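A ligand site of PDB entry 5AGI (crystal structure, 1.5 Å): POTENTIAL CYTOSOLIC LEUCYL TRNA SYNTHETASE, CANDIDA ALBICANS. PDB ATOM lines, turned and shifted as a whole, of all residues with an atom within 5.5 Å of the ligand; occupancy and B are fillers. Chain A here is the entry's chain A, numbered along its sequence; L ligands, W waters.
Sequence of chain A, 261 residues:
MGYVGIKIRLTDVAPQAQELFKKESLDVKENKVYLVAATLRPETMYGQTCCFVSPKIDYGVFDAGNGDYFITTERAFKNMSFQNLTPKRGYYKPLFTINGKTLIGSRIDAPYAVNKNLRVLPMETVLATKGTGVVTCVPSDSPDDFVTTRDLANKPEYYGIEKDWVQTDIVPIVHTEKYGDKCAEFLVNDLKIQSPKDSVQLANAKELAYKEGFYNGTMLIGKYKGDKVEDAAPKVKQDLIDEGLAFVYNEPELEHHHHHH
O of Asp 141 sits close to F1 of the ligand (3.2 Å). A fluorine (F1) of the ligand sits close to the backbone NH of Ser 142 (3.4 Å). O of Ala 38 touches C8 of the ligand (3.4 Å). Arg 41 touches the ligand (CG to C6, 3.7 Å). Thr 44 touches the ligand. Val 126 touches the ligand (CG1 to N3, 3.6 Å). Val 135 touches the ligand (CG2 to C9, 3.4 Å). Val 138 touches the ligand. Hydrophobic or aromatic side chains within 4 Å of the ligand: Leu 40, Val 126, Leu 127, Val 135 and Val 138. Within 4 Å of the ligand: Ala 38, Thr 39, Leu 40, Arg 41, Thr 44, Val 126, Leu 127, Lys 130, Val 135, Val 138, Asp 141, Ser 142 and Lys 206.
Water W4 lies within hydrogen-bond range of the backbone carbonyl oxygen of Ala 38 (2.9 Å), an oxygen (O8) of the ligand (2.9 Å) and the backbone NH of Thr 136 (3.0 Å). Water W9 bridges NZ of Lys 130 (2.9 Å) and O2 of the ligand (3.0 Å). Water W1 lies within hydrogen-bond range of the backbone carbonyl oxygen of Val 134 (2.9 Å), the backbone NH of Thr 132 (2.9 Å), a nitrogen (N2) of the ligand (3.0 Å) and the backbone NH of Gly 133 (3.0 Å). Water W7 bridges the side-chain hydroxyl (OG) of Ser 142 and an oxygen (O7) of the ligand. Water W8 bridges NZ of Lys 206 (2.8 Å) and N5 of the ligand (3.1 Å). Water W6 bridges NH1 of Arg 41 (2.7 Å) and O of Asp 141 (2.7 Å).
The backbone carbonyl oxygen of Leu 127 is in hydrogen-bond range of a nitrogen (N3) of the ligand, 2.9 Å away. O of Lys 130 lies within hydrogen-bond range of N3 of the ligand (3.0 Å). O3 of the ligand is in salt-bridge range of NZ of Lys 130. An oxygen (O2) of the ligand lies within salt-bridge range of the side-chain amino group (NZ) of Lys 206. An oxygen (O6) of the ligand is in hydrogen-bond range of the backbone NH (N) of Leu 40, 3.2 Å away. The backbone NH of Leu 127 lies within hydrogen-bond range of a nitrogen (N4) of the ligand. OG1 of Thr 39 sits at hydrogen-bond distance from O8 of the ligand (2.7 Å).
The side-chain hydroxyl (OG) of Ser 142 lies close to the side-chain carboxylate (OD2) of Asp 145, at 3.2 Å. The backbone NH (N) of Val 138 lies within hydrogen-bond range of the side-chain carboxylate (OD2) of Asp 145 (2.9 Å). OG1 of Thr 44 lies within hydrogen-bond range of O of Arg 41, at 2.7 Å. OG1 of Thr 132 lies within hydrogen-bond range of N of Ala 38 (3.5 Å). OG1 of Thr 39 lies within hydrogen-bond range of N of Arg 41 (2.9 Å). OH of Tyr 3 is in hydrogen-bond range of NZ of Lys 130 (2.7 Å). The backbone NH (N) of Ala 38 is in hydrogen-bond range of the backbone carbonyl oxygen (O) of Val 134, 3.2 Å away.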
ATOM      1  N   TYR A   3      -2.356 -30.696  17.049  1.00  0.00           N
ATOM      2  CA  TYR A   3      -2.788 -29.467  16.408  1.00  0.00           C
ATOM      3  C   TYR A   3      -1.609 -28.528  16.193  1.00  0.00           C
ATOM      4  O   TYR A   3      -0.554 -28.694  16.797  1.00  0.00           O
ATOM      5  CB  TYR A   3      -3.816 -28.736  17.277  1.00  0.00           C
ATOM      6  CG  TYR A   3      -5.104 -29.479  17.494  1.00  0.00           C
ATOM      7  CD1 TYR A   3      -6.158 -29.376  16.595  1.00  0.00           C
ATOM      8  CD2 TYR A   3      -5.280 -30.286  18.615  1.00  0.00           C
ATOM      9  CE1 TYR A   3      -7.341 -30.060  16.790  1.00  0.00           C
ATOM     10  CE2 TYR A   3      -6.455 -30.976  18.820  1.00  0.00           C
ATOM     11  CZ  TYR A   3      -7.486 -30.859  17.911  1.00  0.00           C
ATOM     12  OH  TYR A   3      -8.664 -31.542  18.122  1.00  0.00           O
ATOM     13  N   ALA A  38      -5.961 -23.469  18.403  1.00  0.00           N
ATOM     14  CA  ALA A  38      -5.619 -24.760  17.814  1.00  0.00           C
ATOM     15  C   ALA A  38      -6.227 -24.850  16.428  1.00  0.00           C
ATOM     16  O   ALA A  38      -7.442 -24.685  16.268  1.00  0.00           O
ATOM     17  CB  ALA A  38      -6.130 -25.900  18.692  1.00  0.00           C
ATOM     18  N   THR A  39      -5.386 -25.100  15.423  1.00  0.00           N
ATOM     19  CA  THR A  39      -5.858 -25.240  14.052  1.00  0.00           C
ATOM     20  C   THR A  39      -5.237 -26.461  13.369  1.00  0.00           C
ATOM     21  O   THR A  39      -4.165 -26.927  13.765  1.00  0.00           O
ATOM     22  CB  THR A  39      -5.531 -23.981  13.204  1.00  0.00           C
ATOM     23  OG1 THR A  39      -6.165 -24.093  11.924  1.00  0.00           O
ATOM     24  CG2 THR A  39      -4.027 -23.799  13.000  1.00  0.00           C
ATOM     25  N   LEU A  40      -5.936 -26.973  12.367  1.00  0.00           N
ATOM     26  CA  LEU A  40      -5.385 -27.985  11.461  1.00  0.00           C
ATOM     27  C   LEU A  40      -5.228 -27.419  10.056  1.00  0.00           C
ATOM     28  O   LEU A  40      -4.919 -28.159   9.120  1.00  0.00           O
ATOM     29  CB  LEU A  40      -6.273 -29.229  11.455  1.00  0.00           C
ATOM     30  CG  LEU A  40      -6.369 -30.006  12.771  1.00  0.00           C
ATOM     31  CD1 LEU A  40      -7.285 -31.207  12.626  1.00  0.00           C
ATOM     32  CD2 LEU A  40      -4.986 -30.456  13.245  1.00  0.00           C
ATOM     33  N   ARG A  41      -5.415 -26.104   9.908  1.00  0.00           N
ATOM     34  CA  ARG A  41      -5.376 -25.442   8.605  1.00  0.00           C
ATOM     35  C   ARG A  41      -4.469 -24.204   8.661  1.00  0.00           C
ATOM     36  O   ARG A  41      -4.948 -23.082   8.494  1.00  0.00           O
ATOM     37  CB  ARG A  41      -6.786 -25.044   8.175  1.00  0.00           C
ATOM     38  CG  ARG A  41      -7.783 -26.192   8.120  1.00  0.00           C
ATOM     39  CD  ARG A  41      -7.462 -27.191   7.021  1.00  0.00           C
ATOM     40  NE  ARG A  41      -7.437 -26.560   5.704  1.00  0.00           N
ATOM     41  CZ  ARG A  41      -8.524 -26.208   5.008  1.00  0.00           C
ATOM     42  NH1 ARG A  41      -9.747 -26.412   5.485  1.00  0.00           N
ATOM     43  NH2 ARG A  41      -8.372 -25.633   3.815  1.00  0.00           N
ATOM     44  N   THR A  44      -4.524 -21.227   6.109  1.00  0.00           N
ATOM     45  CA  THR A  44      -5.632 -20.274   6.091  1.00  0.00           C
ATOM     46  C   THR A  44      -5.446 -19.078   7.024  1.00  0.00           C
ATOM     47  O   THR A  44      -6.339 -18.228   7.124  1.00  0.00           O
ATOM     48  CB  THR A  44      -6.972 -20.970   6.451  1.00  0.00           C
ATOM     49  OG1 THR A  44      -6.948 -21.362   7.825  1.00  0.00           O
ATOM     50  CG2 THR A  44      -7.211 -22.176   5.563  1.00  0.00           C
ATOM     51  N   MET A  45      -4.305 -18.994   7.701  1.00  0.00           N
ATOM     52  CA  MET A  45      -4.070 -17.919   8.678  1.00  0.00           C
ATOM     53  C   MET A  45      -4.108 -16.513   8.065  1.00  0.00           C
ATOM     54  O   MET A  45      -4.325 -15.535   8.780  1.00  0.00           O
ATOM     55  CB  MET A  45      -2.736 -18.133   9.418  1.00  0.00           C
ATOM     56  CG  MET A  45      -2.720 -19.329  10.361  1.00  0.00           C
ATOM     57  SD  MET A  45      -4.075 -19.367  11.549  1.00  0.00           S
ATOM     58  CE  MET A  45      -5.246 -20.450  10.734  1.00  0.00           C
ATOM     59  N   MET A 123     -17.711 -17.312  20.775  1.00  0.00           N
ATOM     60  CA  MET A 123     -18.252 -18.446  20.023  1.00  0.00           C
ATOM     61  C   MET A 123     -18.860 -19.424  21.023  1.00  0.00           C
ATOM     62  O   MET A 123     -18.139 -20.010  21.833  1.00  0.00           O
ATOM     63  CB  MET A 123     -17.148 -19.131  19.206  1.00  0.00           C
ATOM     64  CG  MET A 123     -17.572 -20.429  18.531  1.00  0.00           C
ATOM     65  SD  MET A 123     -16.310 -21.105  17.431  1.00  0.00           S
ATOM     66  CE  MET A 123     -16.905 -20.508  15.842  1.00  0.00           C
ATOM     67  N   THR A 125     -20.259 -22.304  20.457  1.00  0.00           N
ATOM     68  CA  THR A 125     -20.148 -23.712  20.064  1.00  0.00           C
ATOM     69  C   THR A 125     -18.721 -24.274  20.134  1.00  0.00           C
ATOM     70  O   THR A 125     -18.421 -25.293  19.506  1.00  0.00           O
ATOM     71  CB  THR A 125     -20.695 -23.912  18.642  1.00  0.00           C
ATOM     72  OG1 THR A 125     -19.989 -23.039  17.735  1.00  0.00           O
ATOM     73  CG2 THR A 125     -22.181 -23.599  18.594  1.00  0.00           C
ATOM     74  N   VAL A 126     -17.846 -23.631  20.902  1.00  0.00           N
ATOM     75  CA  VAL A 126     -16.509 -24.165  21.144  1.00  0.00           C
ATOM     76  C   VAL A 126     -16.626 -25.412  22.019  1.00  0.00           C
ATOM     77  O   VAL A 126     -17.246 -25.367  23.076  1.00  0.00           O
ATOM     78  CB  VAL A 126     -15.591 -23.138  21.837  1.00  0.00           C
ATOM     79  CG1 VAL A 126     -14.274 -23.769  22.256  1.00  0.00           C
ATOM     80  CG2 VAL A 126     -15.339 -21.939  20.939  1.00  0.00           C
ATOM     81  N   LEU A 127     -16.034 -26.516  21.565  1.00  0.00           N
ATOM     82  CA  LEU A 127     -15.997 -27.739  22.362  1.00  0.00           C
ATOM     83  C   LEU A 127     -14.870 -27.608  23.384  1.00  0.00           C
ATOM     84  O   LEU A 127     -13.697 -27.568  23.026  1.00  0.00           O
ATOM     85  CB  LEU A 127     -15.787 -28.957  21.468  1.00  0.00           C
ATOM     86  CG  LEU A 127     -15.834 -30.339  22.122  1.00  0.00           C
ATOM     87  CD1 LEU A 127     -17.114 -30.542  22.923  1.00  0.00           C
ATOM     88  CD2 LEU A 127     -15.714 -31.419  21.060  1.00  0.00           C
ATOM     89  N   ALA A 128     -15.240 -27.529  24.662  1.00  0.00           N
ATOM     90  CA  ALA A 128     -14.286 -27.247  25.742  1.00  0.00           C
ATOM     91  C   ALA A 128     -13.171 -28.284  25.876  1.00  0.00           C
ATOM     92  O   ALA A 128     -12.068 -27.957  26.312  1.00  0.00           O
ATOM     93  CB  ALA A 128     -15.028 -27.090  27.068  1.00  0.00           C
ATOM     94  N   LYS A 130     -11.808 -29.945  23.371  1.00  0.00           N
ATOM     95  CA  LYS A 130     -11.077 -30.050  22.109  1.00  0.00           C
ATOM     96  C   LYS A 130     -10.004 -28.962  22.016  1.00  0.00           C
ATOM     97  O   LYS A 130     -10.275 -27.797  22.301  1.00  0.00           O
ATOM     98  CB  LYS A 130     -12.034 -29.926  20.924  1.00  0.00           C
ATOM     99  CG  LYS A 130     -11.369 -30.040  19.563  1.00  0.00           C
ATOM    100  CD  LYS A 130     -12.391 -29.981  18.442  1.00  0.00           C
ATOM    101  CE  LYS A 130     -11.724 -29.947  17.070  1.00  0.00           C
ATOM    102  NZ  LYS A 130     -11.018 -31.229  16.745  1.00  0.00           N
ATOM    103  N   GLY A 131      -8.800 -29.348  21.625  1.00  0.00           N
ATOM    104  CA  GLY A 131      -7.697 -28.396  21.418  1.00  0.00           C
ATOM    105  C   GLY A 131      -7.437 -27.529  22.636  1.00  0.00           C
ATOM    106  O   GLY A 131      -7.336 -28.032  23.757  1.00  0.00           O
ATOM    107  N   THR A 132      -7.334 -26.220  22.414  1.00  0.00           N
ATOM    108  CA  THR A 132      -7.029 -25.245  23.468  1.00  0.00           C
ATOM    109  C   THR A 132      -8.266 -24.527  24.000  1.00  0.00           C
ATOM    110  O   THR A 132      -8.167 -23.733  24.946  1.00  0.00           O
ATOM    111  CB  THR A 132      -6.067 -24.173  22.940  1.00  0.00           C
ATOM    112  OG1 THR A 132      -6.649 -23.542  21.793  1.00  0.00           O
ATOM    113  CG2 THR A 132      -4.732 -24.781  22.554  1.00  0.00           C
ATOM    114  N   GLY A 133      -9.424 -24.772  23.398  1.00  0.00           N
ATOM    115  CA  GLY A 133     -10.631 -24.008  23.687  1.00  0.00           C
ATOM    116  C   GLY A 133     -10.636 -22.628  23.034  1.00  0.00           C
ATOM    117  O   GLY A 133     -11.540 -21.831  23.271  1.00  0.00           O
ATOM    118  N   VAL A 134      -9.617 -22.359  22.218  1.00  0.00           N
ATOM    119  CA  VAL A 134      -9.481 -21.096  21.502  1.00  0.00           C
ATOM    120  C   VAL A 134      -9.492 -21.433  20.018  1.00  0.00           C
ATOM    121  O   VAL A 134      -8.764 -22.331  19.575  1.00  0.00           O
ATOM    122  CB  VAL A 134      -8.175 -20.362  21.875  1.00  0.00           C
ATOM    123  CG1 VAL A 134      -8.061 -19.031  21.143  1.00  0.00           C
ATOM    124  CG2 VAL A 134      -8.089 -20.154  23.388  1.00  0.00           C
ATOM    125  N   VAL A 135     -10.308 -20.729  19.256  1.00  0.00           N
ATOM    126  CA  VAL A 135     -10.494 -21.016  17.828  1.00  0.00           C
ATOM    127  C   VAL A 135     -10.312 -19.718  17.046  1.00  0.00           C
ATOM    128  O   VAL A 135     -11.005 -18.746  17.296  1.00  0.00           O
ATOM    129  CB  VAL A 135     -11.906 -21.581  17.567  1.00  0.00           C
ATOM    130  CG1 VAL A 135     -12.118 -21.855  16.078  1.00  0.00           C
ATOM    131  CG2 VAL A 135     -12.118 -22.855  18.375  1.00  0.00           C
ATOM    132  N   THR A 136      -9.373 -19.706  16.100  1.00  0.00           N
ATOM    133  CA  THR A 136      -9.199 -18.522  15.264  1.00  0.00           C
ATOM    134  C   THR A 136     -10.209 -18.545  14.120  1.00  0.00           C
ATOM    135  O   THR A 136     -10.600 -19.613  13.645  1.00  0.00           O
ATOM    136  CB  THR A 136      -7.761 -18.360  14.734  1.00  0.00           C
ATOM    137  OG1 THR A 136      -7.585 -17.018  14.269  1.00  0.00           O
ATOM    138  CG2 THR A 136      -7.443 -19.349  13.604  1.00  0.00           C
ATOM    139  N   VAL A 138     -11.717 -17.939  10.514  1.00  0.00           N
ATOM    140  CA  VAL A 138     -11.485 -17.824   9.077  1.00  0.00           C
ATOM    141  C   VAL A 138     -12.817 -18.045   8.342  1.00  0.00           C
ATOM    142  O   VAL A 138     -13.110 -19.162   7.901  1.00  0.00           O
ATOM    143  CB  VAL A 138     -10.423 -18.836   8.587  1.00  0.00           C
ATOM    144  CG1 VAL A 138     -10.099 -18.614   7.124  1.00  0.00           C
ATOM    145  CG2 VAL A 138      -9.154 -18.717   9.435  1.00  0.00           C
ATOM    146  N   ASP A 141     -13.336 -19.965   4.687  1.00  0.00           N
ATOM    147  CA  ASP A 141     -13.165 -21.412   4.507  1.00  0.00           C
ATOM    148  C   ASP A 141     -13.680 -22.310   5.641  1.00  0.00           C
ATOM    149  O   ASP A 141     -13.794 -23.521   5.448  1.00  0.00           O
ATOM    150  CB  ASP A 141     -11.702 -21.723   4.216  1.00  0.00           C
ATOM    151  CG  ASP A 141     -11.248 -21.200   2.877  1.00  0.00           C
ATOM    152  OD1 ASP A 141     -10.963 -19.980   2.777  1.00  0.00           O
ATOM    153  OD2 ASP A 141     -11.209 -21.983   1.916  1.00  0.00           O
ATOM    154  N   SER A 142     -13.996 -21.738   6.803  1.00  0.00           N
ATOM    155  CA  SER A 142     -14.594 -22.502   7.897  1.00  0.00           C
ATOM    156  C   SER A 142     -16.079 -22.203   8.006  1.00  0.00           C
ATOM    157  O   SER A 142     -16.467 -21.077   8.352  1.00  0.00           O
ATOM    158  CB  SER A 142     -13.908 -22.159   9.227  1.00  0.00           C
ATOM    159  OG  SER A 142     -14.663 -22.650  10.323  1.00  0.00           O
ATOM    160  N   ASP A 145     -17.062 -20.869  11.429  1.00  0.00           N
ATOM    161  CA  ASP A 145     -16.637 -19.476  11.611  1.00  0.00           C
ATOM    162  C   ASP A 145     -17.531 -18.514  10.831  1.00  0.00           C
ATOM    163  O   ASP A 145     -17.850 -17.436  11.321  1.00  0.00           O
ATOM    164  CB  ASP A 145     -15.178 -19.298  11.189  1.00  0.00           C
ATOM    165  CG  ASP A 145     -14.217 -20.135  12.031  1.00  0.00           C
ATOM    166  OD1 ASP A 145     -14.628 -20.660  13.094  1.00  0.00           O
ATOM    167  OD2 ASP A 145     -13.050 -20.252  11.624  1.00  0.00           O
ATOM    168  N   LYS A 206     -18.044 -28.598   6.738  1.00  0.00           N
ATOM    169  CA  LYS A 206     -16.638 -28.551   7.131  1.00  0.00           C
ATOM    170  C   LYS A 206     -15.788 -29.542   6.342  1.00  0.00           C
ATOM    171  O   LYS A 206     -14.707 -29.203   5.853  1.00  0.00           O
ATOM    172  CB  LYS A 206     -16.503 -28.820   8.639  1.00  0.00           C
ATOM    173  CG  LYS A 206     -15.111 -28.635   9.203  1.00  0.00           C
ATOM    174  CD  LYS A 206     -15.157 -28.760  10.722  1.00  0.00           C
ATOM    175  CE  LYS A 206     -13.785 -28.538  11.350  1.00  0.00           C
ATOM    176  NZ  LYS A 206     -13.839 -28.778  12.816  1.00  0.00           N
HETATM  177  C1  LIG L   1      -8.747 -22.440  11.198  1.00  0.00           C
HETATM  178  C2  LIG L   1      -9.549 -23.123  10.131  1.00  0.00           C
HETATM  179  C3  LIG L   1      -9.794 -22.693   8.831  1.00  0.00           C
HETATM  180  C4  LIG L   1     -10.053 -24.298  10.608  1.00  0.00           C
HETATM  181  C5  LIG L   1     -10.590 -23.505   8.011  1.00  0.00           C
HETATM  182  C6  LIG L   1     -10.853 -25.108   9.801  1.00  0.00           C
HETATM  183  C7  LIG L   1     -11.114 -24.701   8.492  1.00  0.00           C
HETATM  184  P1  LIG L   1     -11.196 -31.213  13.038  1.00  0.00           P
HETATM  185  O1  LIG L   1     -10.689 -31.837  11.759  1.00  0.00           O
HETATM  186  O2  LIG L   1     -12.677 -31.411  13.273  1.00  0.00           O
HETATM  187  O3  LIG L   1     -10.336 -31.495  14.247  1.00  0.00           O
HETATM  188  N1  LIG L   1     -11.524 -26.086  16.213  1.00  0.00           N
HETATM  189  C8  LIG L   1     -10.389 -26.197  16.929  1.00  0.00           C
HETATM  190  N2  LIG L   1     -10.692 -26.304  18.241  1.00  0.00           N
HETATM  191  C9  LIG L   1     -12.031 -26.265  18.344  1.00  0.00           C
HETATM  192  C10 LIG L   1     -12.910 -26.326  19.431  1.00  0.00           C
HETATM  193  N3  LIG L   1     -12.437 -26.453  20.681  1.00  0.00           N
HETATM  194  N4  LIG L   1     -14.246 -26.261  19.205  1.00  0.00           N
HETATM  195  C11 LIG L   1     -14.722 -26.126  17.960  1.00  0.00           C
HETATM  196  N5  LIG L   1     -13.890 -26.070  16.898  1.00  0.00           N
HETATM  197  C12 LIG L   1     -12.549 -26.129  17.065  1.00  0.00           C
HETATM  198  O4  LIG L   1     -11.083 -29.630  12.777  1.00  0.00           O
HETATM  199  C13 LIG L   1     -10.025 -28.803  13.276  1.00  0.00           C
HETATM  200  C14 LIG L   1     -10.545 -27.375  13.213  1.00  0.00           C
HETATM  201  O5  LIG L   1     -11.651 -27.242  14.123  1.00  0.00           O
HETATM  202  C15 LIG L   1      -9.542 -26.298  13.575  1.00  0.00           C
HETATM  203  O6  LIG L   1      -8.923 -25.695  12.449  1.00  0.00           O
HETATM  204  C16 LIG L   1     -10.452 -25.219  14.137  1.00  0.00           C
HETATM  205  O7  LIG L   1     -10.762 -24.457  12.983  1.00  0.00           O
HETATM  206  C17 LIG L   1     -11.636 -25.947  14.736  1.00  0.00           C
HETATM  207  F1  LIG L   1     -10.852 -23.120   6.749  1.00  0.00           F
HETATM  208  O8  LIG L   1      -8.803 -23.407  12.269  1.00  0.00           O
HETATM  209  B1  LIG L   1      -9.668 -24.556  12.072  1.00  0.00           B
HETATM  210  O   HOH W   1      -9.081 -25.059  20.387  1.00  0.00           O
HETATM  211  O   HOH W   2     -11.540 -21.958  12.991  1.00  0.00           O
HETATM  212  O   HOH W   3      -8.651 -33.894  14.545  1.00  0.00           O
HETATM  213  O   HOH W   4      -8.526 -22.337  14.982  1.00  0.00           O
HETATM  214  O   HOH W   5     -16.850 -24.112  16.064  1.00  0.00           O
HETATM  215  O   HOH W   6     -12.163 -25.553   4.604  1.00  0.00           O
HETATM  216  O   HOH W   7     -13.486 -24.649  11.738  1.00  0.00           O
HETATM  217  O   HOH W   8     -14.964 -26.461  14.015  1.00  0.00           O
HETATM  218  O   HOH W   9     -13.556 -32.420  15.909  1.00  0.00           O
